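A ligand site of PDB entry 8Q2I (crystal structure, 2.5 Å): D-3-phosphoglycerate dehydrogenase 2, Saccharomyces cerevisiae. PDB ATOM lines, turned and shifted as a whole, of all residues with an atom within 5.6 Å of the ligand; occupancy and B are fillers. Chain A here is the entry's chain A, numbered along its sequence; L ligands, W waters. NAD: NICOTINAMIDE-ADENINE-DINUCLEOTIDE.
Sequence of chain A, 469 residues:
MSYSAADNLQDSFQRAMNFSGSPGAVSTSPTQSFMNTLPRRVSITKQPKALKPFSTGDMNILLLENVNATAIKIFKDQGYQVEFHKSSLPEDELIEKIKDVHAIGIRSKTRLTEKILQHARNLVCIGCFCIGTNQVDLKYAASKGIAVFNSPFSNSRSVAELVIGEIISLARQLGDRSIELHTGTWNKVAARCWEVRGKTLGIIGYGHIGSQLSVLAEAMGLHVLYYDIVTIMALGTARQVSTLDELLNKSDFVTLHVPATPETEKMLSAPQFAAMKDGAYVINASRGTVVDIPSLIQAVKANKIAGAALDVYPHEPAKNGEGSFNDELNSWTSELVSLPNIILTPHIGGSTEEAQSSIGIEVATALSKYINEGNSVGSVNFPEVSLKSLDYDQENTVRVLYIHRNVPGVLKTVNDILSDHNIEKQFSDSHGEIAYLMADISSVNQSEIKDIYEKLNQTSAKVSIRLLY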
ATOM      1  N   ILE A 131     -22.910   9.129   6.512  1.00  0.00           N
ATOM      2  CA  ILE A 131     -22.976  10.567   6.322  1.00  0.00           C
ATOM      3  C   ILE A 131     -22.390  10.960   4.949  1.00  0.00           C
ATOM      4  O   ILE A 131     -22.991  11.729   4.220  1.00  0.00           O
ATOM      5  CB  ILE A 131     -22.250  11.288   7.483  1.00  0.00           C
ATOM      6  CG1 ILE A 131     -22.883  10.964   8.829  1.00  0.00           C
ATOM      7  CG2 ILE A 131     -22.184  12.793   7.239  1.00  0.00           C
ATOM      8  CD1 ILE A 131     -22.108  11.473  10.006  1.00  0.00           C
ATOM      9  N   PRO A 152     -27.377  11.892   7.619  1.00  0.00           N
ATOM     10  CA  PRO A 152     -26.485  12.867   8.238  1.00  0.00           C
ATOM     11  C   PRO A 152     -26.401  12.797   9.785  1.00  0.00           C
ATOM     12  O   PRO A 152     -25.312  12.945  10.314  1.00  0.00           O
ATOM     13  CB  PRO A 152     -27.008  14.199   7.677  1.00  0.00           C
ATOM     14  CG  PRO A 152     -28.475  13.967   7.453  1.00  0.00           C
ATOM     15  CD  PRO A 152     -28.615  12.506   7.088  1.00  0.00           C
ATOM     16  N   PHE A 153     -27.541  12.540  10.483  1.00  0.00           N
ATOM     17  CA  PHE A 153     -27.675  12.891  11.896  1.00  0.00           C
ATOM     18  C   PHE A 153     -28.008  11.693  12.796  1.00  0.00           C
ATOM     19  O   PHE A 153     -28.478  11.854  13.916  1.00  0.00           O
ATOM     20  CB  PHE A 153     -28.778  13.941  12.088  1.00  0.00           C
ATOM     21  CG  PHE A 153     -28.529  15.205  11.295  1.00  0.00           C
ATOM     22  CD1 PHE A 153     -27.281  15.830  11.318  1.00  0.00           C
ATOM     23  CD2 PHE A 153     -29.545  15.741  10.486  1.00  0.00           C
ATOM     24  CE1 PHE A 153     -27.052  16.974  10.565  1.00  0.00           C
ATOM     25  CE2 PHE A 153     -29.298  16.884   9.734  1.00  0.00           C
ATOM     26  CZ  PHE A 153     -28.052  17.494   9.776  1.00  0.00           C
ATOM     27  N   ASN A 155     -25.934   9.529  14.157  1.00  0.00           N
ATOM     28  CA  ASN A 155     -24.850   9.135  15.042  1.00  0.00           C
ATOM     29  C   ASN A 155     -24.691  10.111  16.221  1.00  0.00           C
ATOM     30  O   ASN A 155     -23.699  10.036  16.954  1.00  0.00           O
ATOM     31  CB  ASN A 155     -23.498   9.126  14.334  1.00  0.00           C
ATOM     32  CG  ASN A 155     -23.394   8.182  13.149  1.00  0.00           C
ATOM     33  OD1 ASN A 155     -24.144   7.217  13.004  1.00  0.00           O
ATOM     34  ND2 ASN A 155     -22.449   8.456  12.273  1.00  0.00           N
ATOM     35  N   SER A 156     -25.672  10.992  16.435  1.00  0.00           N
ATOM     36  CA  SER A 156     -25.580  12.068  17.398  1.00  0.00           C
ATOM     37  C   SER A 156     -25.475  11.542  18.829  1.00  0.00           C
ATOM     38  O   SER A 156     -24.544  11.855  19.562  1.00  0.00           O
ATOM     39  CB  SER A 156     -26.762  13.036  17.250  1.00  0.00           C
ATOM     40  OG  SER A 156     -26.866  13.574  15.921  1.00  0.00           O
ATOM     41  N   VAL A 159     -22.147   9.730  19.705  1.00  0.00           N
ATOM     42  CA  VAL A 159     -21.005  10.593  19.950  1.00  0.00           C
ATOM     43  C   VAL A 159     -21.144  11.295  21.303  1.00  0.00           C
ATOM     44  O   VAL A 159     -20.165  11.456  22.009  1.00  0.00           O
ATOM     45  CB  VAL A 159     -20.812  11.604  18.795  1.00  0.00           C
ATOM     46  CG1 VAL A 159     -19.751  12.644  19.083  1.00  0.00           C
ATOM     47  CG2 VAL A 159     -20.493  10.905  17.481  1.00  0.00           C
ATOM     48  N   ILE A 204     -17.982  23.548  21.853  1.00  0.00           N
ATOM     49  CA  ILE A 204     -17.764  24.323  20.653  1.00  0.00           C
ATOM     50  C   ILE A 204     -18.564  23.700  19.510  1.00  0.00           C
ATOM     51  O   ILE A 204     -18.230  22.637  19.005  1.00  0.00           O
ATOM     52  CB  ILE A 204     -16.251  24.411  20.353  1.00  0.00           C
ATOM     53  CG1 ILE A 204     -15.480  25.028  21.530  1.00  0.00           C
ATOM     54  CG2 ILE A 204     -16.006  25.153  19.042  1.00  0.00           C
ATOM     55  CD1 ILE A 204     -13.983  24.907  21.409  1.00  0.00           C
ATOM     56  N   GLY A 205     -19.679  24.356  19.158  1.00  0.00           N
ATOM     57  CA  GLY A 205     -20.582  23.850  18.151  1.00  0.00           C
ATOM     58  C   GLY A 205     -21.806  23.214  18.790  1.00  0.00           C
ATOM     59  O   GLY A 205     -21.757  22.042  19.136  1.00  0.00           O
ATOM     60  N   TYR A 206     -22.886  24.006  18.920  1.00  0.00           N
ATOM     61  CA  TYR A 206     -24.117  23.595  19.582  1.00  0.00           C
ATOM     62  C   TYR A 206     -25.140  23.099  18.559  1.00  0.00           C
ATOM     63  O   TYR A 206     -26.294  23.569  18.546  1.00  0.00           O
ATOM     64  CB  TYR A 206     -24.667  24.735  20.422  1.00  0.00           C
ATOM     65  CG  TYR A 206     -25.528  24.362  21.608  1.00  0.00           C
ATOM     66  CD1 TYR A 206     -24.967  23.885  22.795  1.00  0.00           C
ATOM     67  CD2 TYR A 206     -26.921  24.560  21.583  1.00  0.00           C
ATOM     68  CE1 TYR A 206     -25.759  23.596  23.900  1.00  0.00           C
ATOM     69  CE2 TYR A 206     -27.705  24.289  22.698  1.00  0.00           C
ATOM     70  CZ  TYR A 206     -27.127  23.802  23.863  1.00  0.00           C
ATOM     71  OH  TYR A 206     -27.869  23.559  24.997  1.00  0.00           O
ATOM     72  N   GLY A 207     -24.745  22.063  17.795  1.00  0.00           N
ATOM     73  CA  GLY A 207     -25.572  21.474  16.749  1.00  0.00           C
ATOM     74  C   GLY A 207     -26.332  20.255  17.248  1.00  0.00           C
ATOM     75  O   GLY A 207     -26.832  20.244  18.373  1.00  0.00           O
ATOM     76  N   HIS A 208     -26.426  19.243  16.400  1.00  0.00           N
ATOM     77  CA  HIS A 208     -27.186  18.016  16.770  1.00  0.00           C
ATOM     78  C   HIS A 208     -26.483  17.324  17.924  1.00  0.00           C
ATOM     79  O   HIS A 208     -27.161  16.986  18.896  1.00  0.00           O
ATOM     80  CB  HIS A 208     -27.327  17.124  15.538  1.00  0.00           C
ATOM     81  CG  HIS A 208     -28.466  17.484  14.655  1.00  0.00           C
ATOM     82  ND1 HIS A 208     -28.299  18.109  13.434  1.00  0.00           N
ATOM     83  CD2 HIS A 208     -29.804  17.314  14.804  1.00  0.00           C
ATOM     84  CE1 HIS A 208     -29.474  18.298  12.870  1.00  0.00           C
ATOM     85  NE2 HIS A 208     -30.410  17.816  13.691  1.00  0.00           N
ATOM     86  N   ILE A 209     -25.182  17.139  17.834  1.00  0.00           N
ATOM     87  CA  ILE A 209     -24.401  16.477  18.872  1.00  0.00           C
ATOM     88  C   ILE A 209     -24.211  17.399  20.073  1.00  0.00           C
ATOM     89  O   ILE A 209     -24.421  16.992  21.200  1.00  0.00           O
ATOM     90  CB  ILE A 209     -23.034  16.031  18.314  1.00  0.00           C
ATOM     91  CG1 ILE A 209     -23.175  14.992  17.191  1.00  0.00           C
ATOM     92  CG2 ILE A 209     -22.155  15.548  19.448  1.00  0.00           C
ATOM     93  CD1 ILE A 209     -21.933  14.649  16.452  1.00  0.00           C
ATOM     94  N   GLY A 210     -23.788  18.635  19.835  1.00  0.00           N
ATOM     95  CA  GLY A 210     -23.521  19.563  20.917  1.00  0.00           C
ATOM     96  C   GLY A 210     -24.734  19.767  21.823  1.00  0.00           C
ATOM     97  O   GLY A 210     -24.568  19.848  23.027  1.00  0.00           O
ATOM     98  N   TYR A 227     -19.914  27.933  22.634  1.00  0.00           N
ATOM     99  CA  TYR A 227     -19.597  28.902  21.603  1.00  0.00           C
ATOM    100  C   TYR A 227     -20.078  28.357  20.262  1.00  0.00           C
ATOM    101  O   TYR A 227     -19.755  27.229  19.912  1.00  0.00           O
ATOM    102  CB  TYR A 227     -18.109  29.244  21.578  1.00  0.00           C
ATOM    103  CG  TYR A 227     -17.758  30.186  20.452  1.00  0.00           C
ATOM    104  CD1 TYR A 227     -17.651  29.697  19.163  1.00  0.00           C
ATOM    105  CD2 TYR A 227     -17.640  31.560  20.641  1.00  0.00           C
ATOM    106  CE1 TYR A 227     -17.371  30.545  18.094  1.00  0.00           C
ATOM    107  CE2 TYR A 227     -17.343  32.405  19.587  1.00  0.00           C
ATOM    108  CZ  TYR A 227     -17.157  31.888  18.316  1.00  0.00           C
ATOM    109  OH  TYR A 227     -16.890  32.698  17.229  1.00  0.00           O
ATOM    110  N   ASP A 228     -20.844  29.172  19.522  1.00  0.00           N
ATOM    111  CA  ASP A 228     -21.197  28.879  18.145  1.00  0.00           C
ATOM    112  C   ASP A 228     -21.090  30.182  17.347  1.00  0.00           C
ATOM    113  O   ASP A 228     -21.058  31.272  17.926  1.00  0.00           O
ATOM    114  CB  ASP A 228     -22.599  28.271  18.079  1.00  0.00           C
ATOM    115  CG  ASP A 228     -22.845  27.454  16.827  1.00  0.00           C
ATOM    116  OD1 ASP A 228     -22.787  28.032  15.734  1.00  0.00           O
ATOM    117  OD2 ASP A 228     -23.098  26.248  16.964  1.00  0.00           O
ATOM    118  N   ILE A 229     -21.001  30.081  16.009  1.00  0.00           N
ATOM    119  CA  ILE A 229     -20.931  31.254  15.151  1.00  0.00           C
ATOM    120  C   ILE A 229     -22.338  31.799  14.887  1.00  0.00           C
ATOM    121  O   ILE A 229     -22.507  32.803  14.224  1.00  0.00           O
ATOM    122  CB  ILE A 229     -20.167  30.970  13.841  1.00  0.00           C
ATOM    123  CG1 ILE A 229     -20.818  29.868  12.995  1.00  0.00           C
ATOM    124  CG2 ILE A 229     -18.696  30.682  14.126  1.00  0.00           C
ATOM    125  CD1 ILE A 229     -20.226  29.765  11.593  1.00  0.00           C
ATOM    126  N   VAL A 230     -23.354  31.147  15.449  1.00  0.00           N
ATOM    127  CA  VAL A 230     -24.744  31.535  15.271  1.00  0.00           C
ATOM    128  C   VAL A 230     -25.360  31.620  16.664  1.00  0.00           C
ATOM    129  O   VAL A 230     -24.929  30.914  17.569  1.00  0.00           O
ATOM    130  CB  VAL A 230     -25.437  30.487  14.381  1.00  0.00           C
ATOM    131  CG1 VAL A 230     -26.948  30.412  14.583  1.00  0.00           C
ATOM    132  CG2 VAL A 230     -25.077  30.700  12.924  1.00  0.00           C
ATOM    133  N   ILE A 232     -27.981  30.534  19.098  1.00  0.00           N
ATOM    134  CA  ILE A 232     -28.767  29.314  19.218  1.00  0.00           C
ATOM    135  C   ILE A 232     -29.428  29.336  20.581  1.00  0.00           C
ATOM    136  O   ILE A 232     -28.750  29.601  21.560  1.00  0.00           O
ATOM    137  CB  ILE A 232     -27.856  28.084  19.021  1.00  0.00           C
ATOM    138  CG1 ILE A 232     -27.133  28.125  17.676  1.00  0.00           C
ATOM    139  CG2 ILE A 232     -28.665  26.805  19.219  1.00  0.00           C
ATOM    140  CD1 ILE A 232     -26.059  27.076  17.462  1.00  0.00           C
ATOM    141  N   HIS A 257     -17.576  20.018  18.429  1.00  0.00           N
ATOM    142  CA  HIS A 257     -18.669  19.388  17.645  1.00  0.00           C
ATOM    143  C   HIS A 257     -18.990  20.318  16.464  1.00  0.00           C
ATOM    144  O   HIS A 257     -20.151  20.660  16.291  1.00  0.00           O
ATOM    145  CB  HIS A 257     -19.836  19.082  18.571  1.00  0.00           C
ATOM    146  CG  HIS A 257     -19.419  18.188  19.687  1.00  0.00           C
ATOM    147  ND1 HIS A 257     -19.028  16.892  19.480  1.00  0.00           N
ATOM    148  CD2 HIS A 257     -19.284  18.420  21.011  1.00  0.00           C
ATOM    149  CE1 HIS A 257     -18.686  16.342  20.619  1.00  0.00           C
ATOM    150  NE2 HIS A 257     -18.830  17.262  21.572  1.00  0.00           N
ATOM    151  N   VAL A 258     -17.989  20.651  15.667  1.00  0.00           N
ATOM    152  CA  VAL A 258     -18.078  21.592  14.534  1.00  0.00           C
ATOM    153  C   VAL A 258     -17.843  20.860  13.200  1.00  0.00           C
ATOM    154  O   VAL A 258     -17.198  19.818  13.131  1.00  0.00           O
ATOM    155  CB  VAL A 258     -17.055  22.738  14.664  1.00  0.00           C
ATOM    156  CG1 VAL A 258     -17.321  23.600  15.900  1.00  0.00           C
ATOM    157  CG2 VAL A 258     -15.608  22.252  14.652  1.00  0.00           C
ATOM    158  N   PRO A 259     -18.329  21.423  12.069  1.00  0.00           N
ATOM    159  CA  PRO A 259     -17.944  20.933  10.734  1.00  0.00           C
ATOM    160  C   PRO A 259     -16.504  21.301  10.355  1.00  0.00           C
ATOM    161  O   PRO A 259     -15.872  22.116  11.042  1.00  0.00           O
ATOM    162  CB  PRO A 259     -18.973  21.612   9.822  1.00  0.00           C
ATOM    163  CG  PRO A 259     -19.350  22.902  10.535  1.00  0.00           C
ATOM    164  CD  PRO A 259     -19.287  22.533  12.007  1.00  0.00           C
ATOM    165  N   ALA A 260     -15.980  20.670   9.296  1.00  0.00           N
ATOM    166  CA  ALA A 260     -14.699  21.057   8.696  1.00  0.00           C
ATOM    167  C   ALA A 260     -14.925  22.195   7.701  1.00  0.00           C
ATOM    168  O   ALA A 260     -15.499  22.000   6.632  1.00  0.00           O
ATOM    169  CB  ALA A 260     -13.996  19.867   8.059  1.00  0.00           C
ATOM    170  N   THR A 261     -14.559  23.410   8.122  1.00  0.00           N
ATOM    171  CA  THR A 261     -14.597  24.615   7.303  1.00  0.00           C
ATOM    172  C   THR A 261     -13.180  25.187   7.357  1.00  0.00           C
ATOM    173  O   THR A 261     -12.331  24.657   8.078  1.00  0.00           O
ATOM    174  CB  THR A 261     -15.730  25.591   7.720  1.00  0.00           C
ATOM    175  OG1 THR A 261     -15.434  26.292   8.943  1.00  0.00           O
ATOM    176  CG2 THR A 261     -17.075  24.904   7.880  1.00  0.00           C
ATOM    177  N   GLU A 263     -12.526  27.959   8.715  1.00  0.00           N
ATOM    178  CA  GLU A 263     -12.573  28.647   9.995  1.00  0.00           C
ATOM    179  C   GLU A 263     -12.318  27.681  11.171  1.00  0.00           C
ATOM    180  O   GLU A 263     -11.746  28.091  12.203  1.00  0.00           O
ATOM    181  CB  GLU A 263     -13.941  29.306  10.253  1.00  0.00           C
ATOM    182  CG  GLU A 263     -14.326  30.414   9.287  1.00  0.00           C
ATOM    183  CD  GLU A 263     -14.725  30.035   7.862  1.00  0.00           C
ATOM    184  OE1 GLU A 263     -15.806  29.379   7.645  1.00  0.00           O
ATOM    185  OE2 GLU A 263     -13.943  30.384   6.935  1.00  0.00           O
ATOM    186  N   THR A 264     -12.753  26.416  11.041  1.00  0.00           N
ATOM    187  CA  THR A 264     -12.513  25.394  12.059  1.00  0.00           C
ATOM    188  C   THR A 264     -11.158  24.712  11.855  1.00  0.00           C
ATOM    189  O   THR A 264     -10.640  24.102  12.767  1.00  0.00           O
ATOM    190  CB  THR A 264     -13.633  24.346  12.075  1.00  0.00           C
ATOM    191  OG1 THR A 264     -13.467  23.473  10.943  1.00  0.00           O
ATOM    192  CG2 THR A 264     -15.001  24.984  12.116  1.00  0.00           C
ATOM    193  N   MET A 267      -8.605  25.308  14.569  1.00  0.00           N
ATOM    194  CA  MET A 267      -9.143  26.374  15.399  1.00  0.00           C
ATOM    195  C   MET A 267      -8.680  26.252  16.867  1.00  0.00           C
ATOM    196  O   MET A 267      -8.643  27.267  17.564  1.00  0.00           O
ATOM    197  CB  MET A 267     -10.672  26.432  15.326  1.00  0.00           C
ATOM    198  CG  MET A 267     -11.377  25.262  15.896  1.00  0.00           C
ATOM    199  SD  MET A 267     -13.177  25.424  15.826  1.00  0.00           S
ATOM    200  CE  MET A 267     -13.456  26.977  16.688  1.00  0.00           C
ATOM    201  N   ALA A 285     -14.008  14.733  19.075  1.00  0.00           N
ATOM    202  CA  ALA A 285     -14.671  13.777  18.191  1.00  0.00           C
ATOM    203  C   ALA A 285     -15.450  14.463  17.063  1.00  0.00           C
ATOM    204  O   ALA A 285     -16.513  13.952  16.644  1.00  0.00           O
ATOM    205  CB  ALA A 285     -15.588  12.912  19.033  1.00  0.00           C
ATOM    206  N   SER A 286     -14.950  15.611  16.551  1.00  0.00           N
ATOM    207  CA  SER A 286     -15.573  16.274  15.416  1.00  0.00           C
ATOM    208  C   SER A 286     -14.854  15.853  14.138  1.00  0.00           C
ATOM    209  O   SER A 286     -15.205  14.830  13.570  1.00  0.00           O
ATOM    210  CB  SER A 286     -15.683  17.787  15.584  1.00  0.00           C
ATOM    211  OG  SER A 286     -14.417  18.437  15.689  1.00  0.00           O
ATOM    212  N   ARG A 287     -13.804  16.594  13.759  1.00  0.00           N
ATOM    213  CA  ARG A 287     -13.077  16.370  12.514  1.00  0.00           C
ATOM    214  C   ARG A 287     -11.574  16.362  12.758  1.00  0.00           C
ATOM    215  O   ARG A 287     -11.088  17.103  13.611  1.00  0.00           O
ATOM    216  CB  ARG A 287     -13.384  17.518  11.547  1.00  0.00           C
ATOM    217  CG  ARG A 287     -14.837  17.563  11.124  1.00  0.00           C
ATOM    218  CD  ARG A 287     -15.115  16.250  10.427  1.00  0.00           C
ATOM    219  NE  ARG A 287     -16.368  16.313   9.731  1.00  0.00           N
ATOM    220  CZ  ARG A 287     -16.479  16.256   8.410  1.00  0.00           C
ATOM    221  NH1 ARG A 287     -15.416  16.170   7.630  1.00  0.00           N
ATOM    222  NH2 ARG A 287     -17.689  16.286   7.881  1.00  0.00           N
ATOM    223  N   ASP A 311     -10.867  11.214  18.762  1.00  0.00           N
ATOM    224  CA  ASP A 311     -11.506  10.187  17.968  1.00  0.00           C
ATOM    225  C   ASP A 311     -11.101  10.300  16.499  1.00  0.00           C
ATOM    226  O   ASP A 311     -11.297   9.332  15.741  1.00  0.00           O
ATOM    227  CB  ASP A 311     -13.025  10.247  18.088  1.00  0.00           C
ATOM    228  CG  ASP A 311     -13.729   8.986  17.570  1.00  0.00           C
ATOM    229  OD1 ASP A 311     -13.283   7.862  17.936  1.00  0.00           O
ATOM    230  OD2 ASP A 311     -14.722   9.129  16.817  1.00  0.00           O
ATOM    231  N   VAL A 312     -10.515  11.452  16.089  1.00  0.00           N
ATOM    232  CA  VAL A 312     -10.355  11.785  14.680  1.00  0.00           C
ATOM    233  C   VAL A 312      -8.965  12.372  14.507  1.00  0.00           C
ATOM    234  O   VAL A 312      -8.483  13.046  15.402  1.00  0.00           O
ATOM    235  CB  VAL A 312     -11.448  12.752  14.212  1.00  0.00           C
ATOM    236  CG1 VAL A 312     -12.786  12.067  14.123  1.00  0.00           C
ATOM    237  CG2 VAL A 312     -11.540  14.004  15.088  1.00  0.00           C
ATOM    238  N   HIS A 347     -11.969   6.563  15.368  1.00  0.00           N
ATOM    239  CA  HIS A 347     -13.150   7.073  14.689  1.00  0.00           C
ATOM    240  C   HIS A 347     -14.344   6.174  14.995  1.00  0.00           C
ATOM    241  O   HIS A 347     -15.057   5.744  14.093  1.00  0.00           O
ATOM    242  CB  HIS A 347     -12.848   7.198  13.176  1.00  0.00           C
ATOM    243  CG  HIS A 347     -13.674   8.231  12.450  1.00  0.00           C
ATOM    244  ND1 HIS A 347     -13.187   9.076  11.485  1.00  0.00           N
ATOM    245  CD2 HIS A 347     -14.999   8.508  12.573  1.00  0.00           C
ATOM    246  CE1 HIS A 347     -14.171   9.857  11.051  1.00  0.00           C
ATOM    247  NE2 HIS A 347     -15.317   9.500  11.671  1.00  0.00           N
ATOM    248  N   ILE A 348     -14.586   5.965  16.297  1.00  0.00           N
ATOM    249  CA  ILE A 348     -15.674   5.101  16.745  1.00  0.00           C
ATOM    250  C   ILE A 348     -16.823   5.940  17.308  1.00  0.00           C
ATOM    251  O   ILE A 348     -17.762   5.393  17.878  1.00  0.00           O
ATOM    252  CB  ILE A 348     -15.166   4.009  17.715  1.00  0.00           C
ATOM    253  CG1 ILE A 348     -14.373   4.538  18.923  1.00  0.00           C
ATOM    254  CG2 ILE A 348     -14.305   3.016  16.970  1.00  0.00           C
ATOM    255  CD1 ILE A 348     -15.171   5.381  19.892  1.00  0.00           C
ATOM    256  N   GLY A 349     -16.817   7.254  17.109  1.00  0.00           N
ATOM    257  CA  GLY A 349     -17.860   8.111  17.662  1.00  0.00           C
ATOM    258  C   GLY A 349     -19.279   7.648  17.315  1.00  0.00           C
ATOM    259  O   GLY A 349     -20.149   7.693  18.178  1.00  0.00           O
ATOM    260  N   GLY A 350     -19.495   7.171  16.073  1.00  0.00           N
ATOM    261  CA  GLY A 350     -20.789   6.670  15.637  1.00  0.00           C
ATOM    262  C   GLY A 350     -20.861   5.132  15.506  1.00  0.00           C
ATOM    263  O   GLY A 350     -21.891   4.610  15.065  1.00  0.00           O
HETATM  264  PA  NAD L   1     -24.133  20.207  13.060  1.00  0.00           P
HETATM  265  O1A NAD L   1     -23.959  20.746  11.671  1.00  0.00           O
HETATM  266  O2A NAD L   1     -25.502  19.961  13.634  1.00  0.00           O
HETATM  267  O5B NAD L   1     -23.306  21.113  14.076  1.00  0.00           O
HETATM  268  C5B NAD L   1     -22.272  22.051  13.780  1.00  0.00           C
HETATM  269  C4B NAD L   1     -22.474  23.218  14.708  1.00  0.00           C
HETATM  270  O4B NAD L   1     -21.225  23.962  14.796  1.00  0.00           O
HETATM  271  C3B NAD L   1     -23.582  24.218  14.280  1.00  0.00           C
HETATM  272  O3B NAD L   1     -24.473  24.645  15.320  1.00  0.00           O
HETATM  273  C2B NAD L   1     -22.727  25.295  13.585  1.00  0.00           C
HETATM  274  O2B NAD L   1     -23.350  26.552  13.491  1.00  0.00           O
HETATM  275  C1B NAD L   1     -21.487  25.317  14.485  1.00  0.00           C
HETATM  276  N9A NAD L   1     -20.277  25.852  13.896  1.00  0.00           N
HETATM  277  C8A NAD L   1     -19.867  25.794  12.590  1.00  0.00           C
HETATM  278  N7A NAD L   1     -18.682  26.333  12.393  1.00  0.00           N
HETATM  279  C5A NAD L   1     -18.291  26.742  13.651  1.00  0.00           C
HETATM  280  C6A NAD L   1     -17.115  27.378  14.095  1.00  0.00           C
HETATM  281  N6A NAD L   1     -16.131  27.717  13.270  1.00  0.00           N
HETATM  282  N1A NAD L   1     -17.034  27.666  15.432  1.00  0.00           N
HETATM  283  C2A NAD L   1     -18.058  27.327  16.228  1.00  0.00           C
HETATM  284  N3A NAD L   1     -19.199  26.707  15.922  1.00  0.00           N
HETATM  285  C4A NAD L   1     -19.250  26.444  14.596  1.00  0.00           C
HETATM  286  O3  NAD L   1     -23.291  18.841  13.115  1.00  0.00           O
HETATM  287  PN  NAD L   1     -23.363  17.562  14.088  1.00  0.00           P
HETATM  288  O1N NAD L   1     -24.330  16.525  13.601  1.00  0.00           O
HETATM  289  O2N NAD L   1     -23.545  18.154  15.446  1.00  0.00           O
HETATM  290  O5D NAD L   1     -21.865  17.038  13.864  1.00  0.00           O
HETATM  291  C5D NAD L   1     -20.808  17.813  14.474  1.00  0.00           C
HETATM  292  C4D NAD L   1     -19.500  17.265  13.973  1.00  0.00           C
HETATM  293  O4D NAD L   1     -19.379  15.893  14.387  1.00  0.00           O
HETATM  294  C3D NAD L   1     -19.377  17.227  12.444  1.00  0.00           C
HETATM  295  O3D NAD L   1     -18.013  17.412  12.054  1.00  0.00           O
HETATM  296  C2D NAD L   1     -19.890  15.831  12.131  1.00  0.00           C
HETATM  297  O2D NAD L   1     -19.472  15.478  10.836  1.00  0.00           O
HETATM  298  C1D NAD L   1     -19.145  15.071  13.241  1.00  0.00           C
HETATM  299  N1N NAD L   1     -19.452  13.611  13.551  1.00  0.00           N
HETATM  300  C2N NAD L   1     -18.420  12.751  13.897  1.00  0.00           C
HETATM  301  C3N NAD L   1     -18.662  11.395  14.193  1.00  0.00           C
HETATM  302  C7N NAD L   1     -17.518  10.489  14.577  1.00  0.00           C
HETATM  303  O7N NAD L   1     -17.529   9.304  14.179  1.00  0.00           O
HETATM  304  N7N NAD L   1     -16.498  10.982  15.278  1.00  0.00           N
HETATM  305  C4N NAD L   1     -19.952  10.896  14.079  1.00  0.00           C
HETATM  306  C5N NAD L   1     -20.989  11.758  13.755  1.00  0.00           C
HETATM  307  C6N NAD L   1     -20.737  13.101  13.486  1.00  0.00           C
HETATM  308  O   HOH W   1     -18.592  15.384  17.142  1.00  0.00           O
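Ile 131 touches the ligand. Phe 153 touches the ligand. CB of Asn 155 touches C5N of the ligand, at 3.7 Å. Val 159 touches the ligand (CG2 to C4N, 3.4 Å). Gly 205 touches the ligand. Tyr 206 touches the ligand. CA of Gly 207 touches O2A of the ligand, 3.5 Å away. Tyr 227 touches the ligand (CE1 to C2A, 3.8 Å). Ile 229 touches the ligand. CD1 of Ile 232 touches O3B of the ligand, at 3.6 Å. His 257 touches the ligand (O to C5D, 3.4 Å). Pro 259 touches the ligand. CG2 of Thr 264 touches N6A of the ligand, at 3.2 Å. Met 267 touches the ligand (CE to N1A, 3.9 Å). Ser 286 touches the ligand (O to C2N, 3.8 Å). Gly 349 touches the ligand. Within 4 Å of the ligand: Ile 131, Phe 153, Asn 155, Val 159, Gly 205, Tyr 206, Gly 207, His 208, Ile 209, Tyr 227, Asp 228, Ile 229, Ile 232, His 257, Val 258, Pro 259, Thr 264, Met 267, Ala 285, Ser 286, Arg 287, Asp 311, His 347, Gly 349 and Gly 350. Along chain A the residues within 4 Å of the ligand span positions 131 to 350. The nearest printed residue that does not touch the ligand is Val 312 (4.04 Å).
The backbone NH of Ile 348 sits at hydrogen-bond distance from the side-chain carboxylate of Asp 311 (2.8 Å). The backbone NH (N) of His 347 is in hydrogen-bond range of the backbone carbonyl oxygen (O) of Asp 311, at 2.9 Å. O of Phe 153 lies within hydrogen-bond range of OG of Ser 156 (3.1 Å). OD1 of Asp 228 lies close to N of Val 230, 3.2 Å away. The backbone NH (N) of Gly 205 sits at hydrogen-bond distance from the backbone carbonyl oxygen (O) of Tyr 227 (3.0 Å). The backbone NH (N) of Val 159 sits at hydrogen-bond distance from the backbone carbonyl oxygen (O) of Gly 349, 3.2 Å away. The backbone NH of Gly 349 sits at hydrogen-bond distance from the side-chain carboxylate of Asp 311 (2.8 Å). The backbone carbonyl oxygen (O) of Ile 204 is in hydrogen-bond range of the backbone NH (N) of His 257, 2.8 Å away.
The backbone NH of Gly 350 lies within hydrogen-bond range of an oxygen (O7N) of the ligand (3.5 Å). The backbone carbonyl oxygen of Val 258 sits at hydrogen-bond distance from an oxygen (O3D) of the ligand (2.8 Å). An oxygen (O3D) of the ligand sits at hydrogen-bond distance from the guanidinium group (NE) of Arg 287, 3.1 Å away. O of Ala 285 is in hydrogen-bond range of N7N of the ligand. A nitrogen (N7N) of the ligand lies within hydrogen-bond range of the side-chain carboxylate of Asp 311 (3.0 Å). N of His 208 lies within hydrogen-bond range of O2A of the ligand (3.0 Å). An oxygen (O2N) of the ligand is in hydrogen-bond range of the backbone NH of Ile 209, at 3.1 Å. An oxygen (O3B) of the ligand is in hydrogen-bond range of the side-chain carboxylate (OD2) of Asp 228, 2.7 Å away. O7N of the ligand sits close to NE2 of His 347. ND1 of His 208 is in hydrogen-bond range of O2A of the ligand (3.4 Å).
Water W1 lies within hydrogen-bond range of O of Ala 285, ND1 of His 257 and O4D of the ligand.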
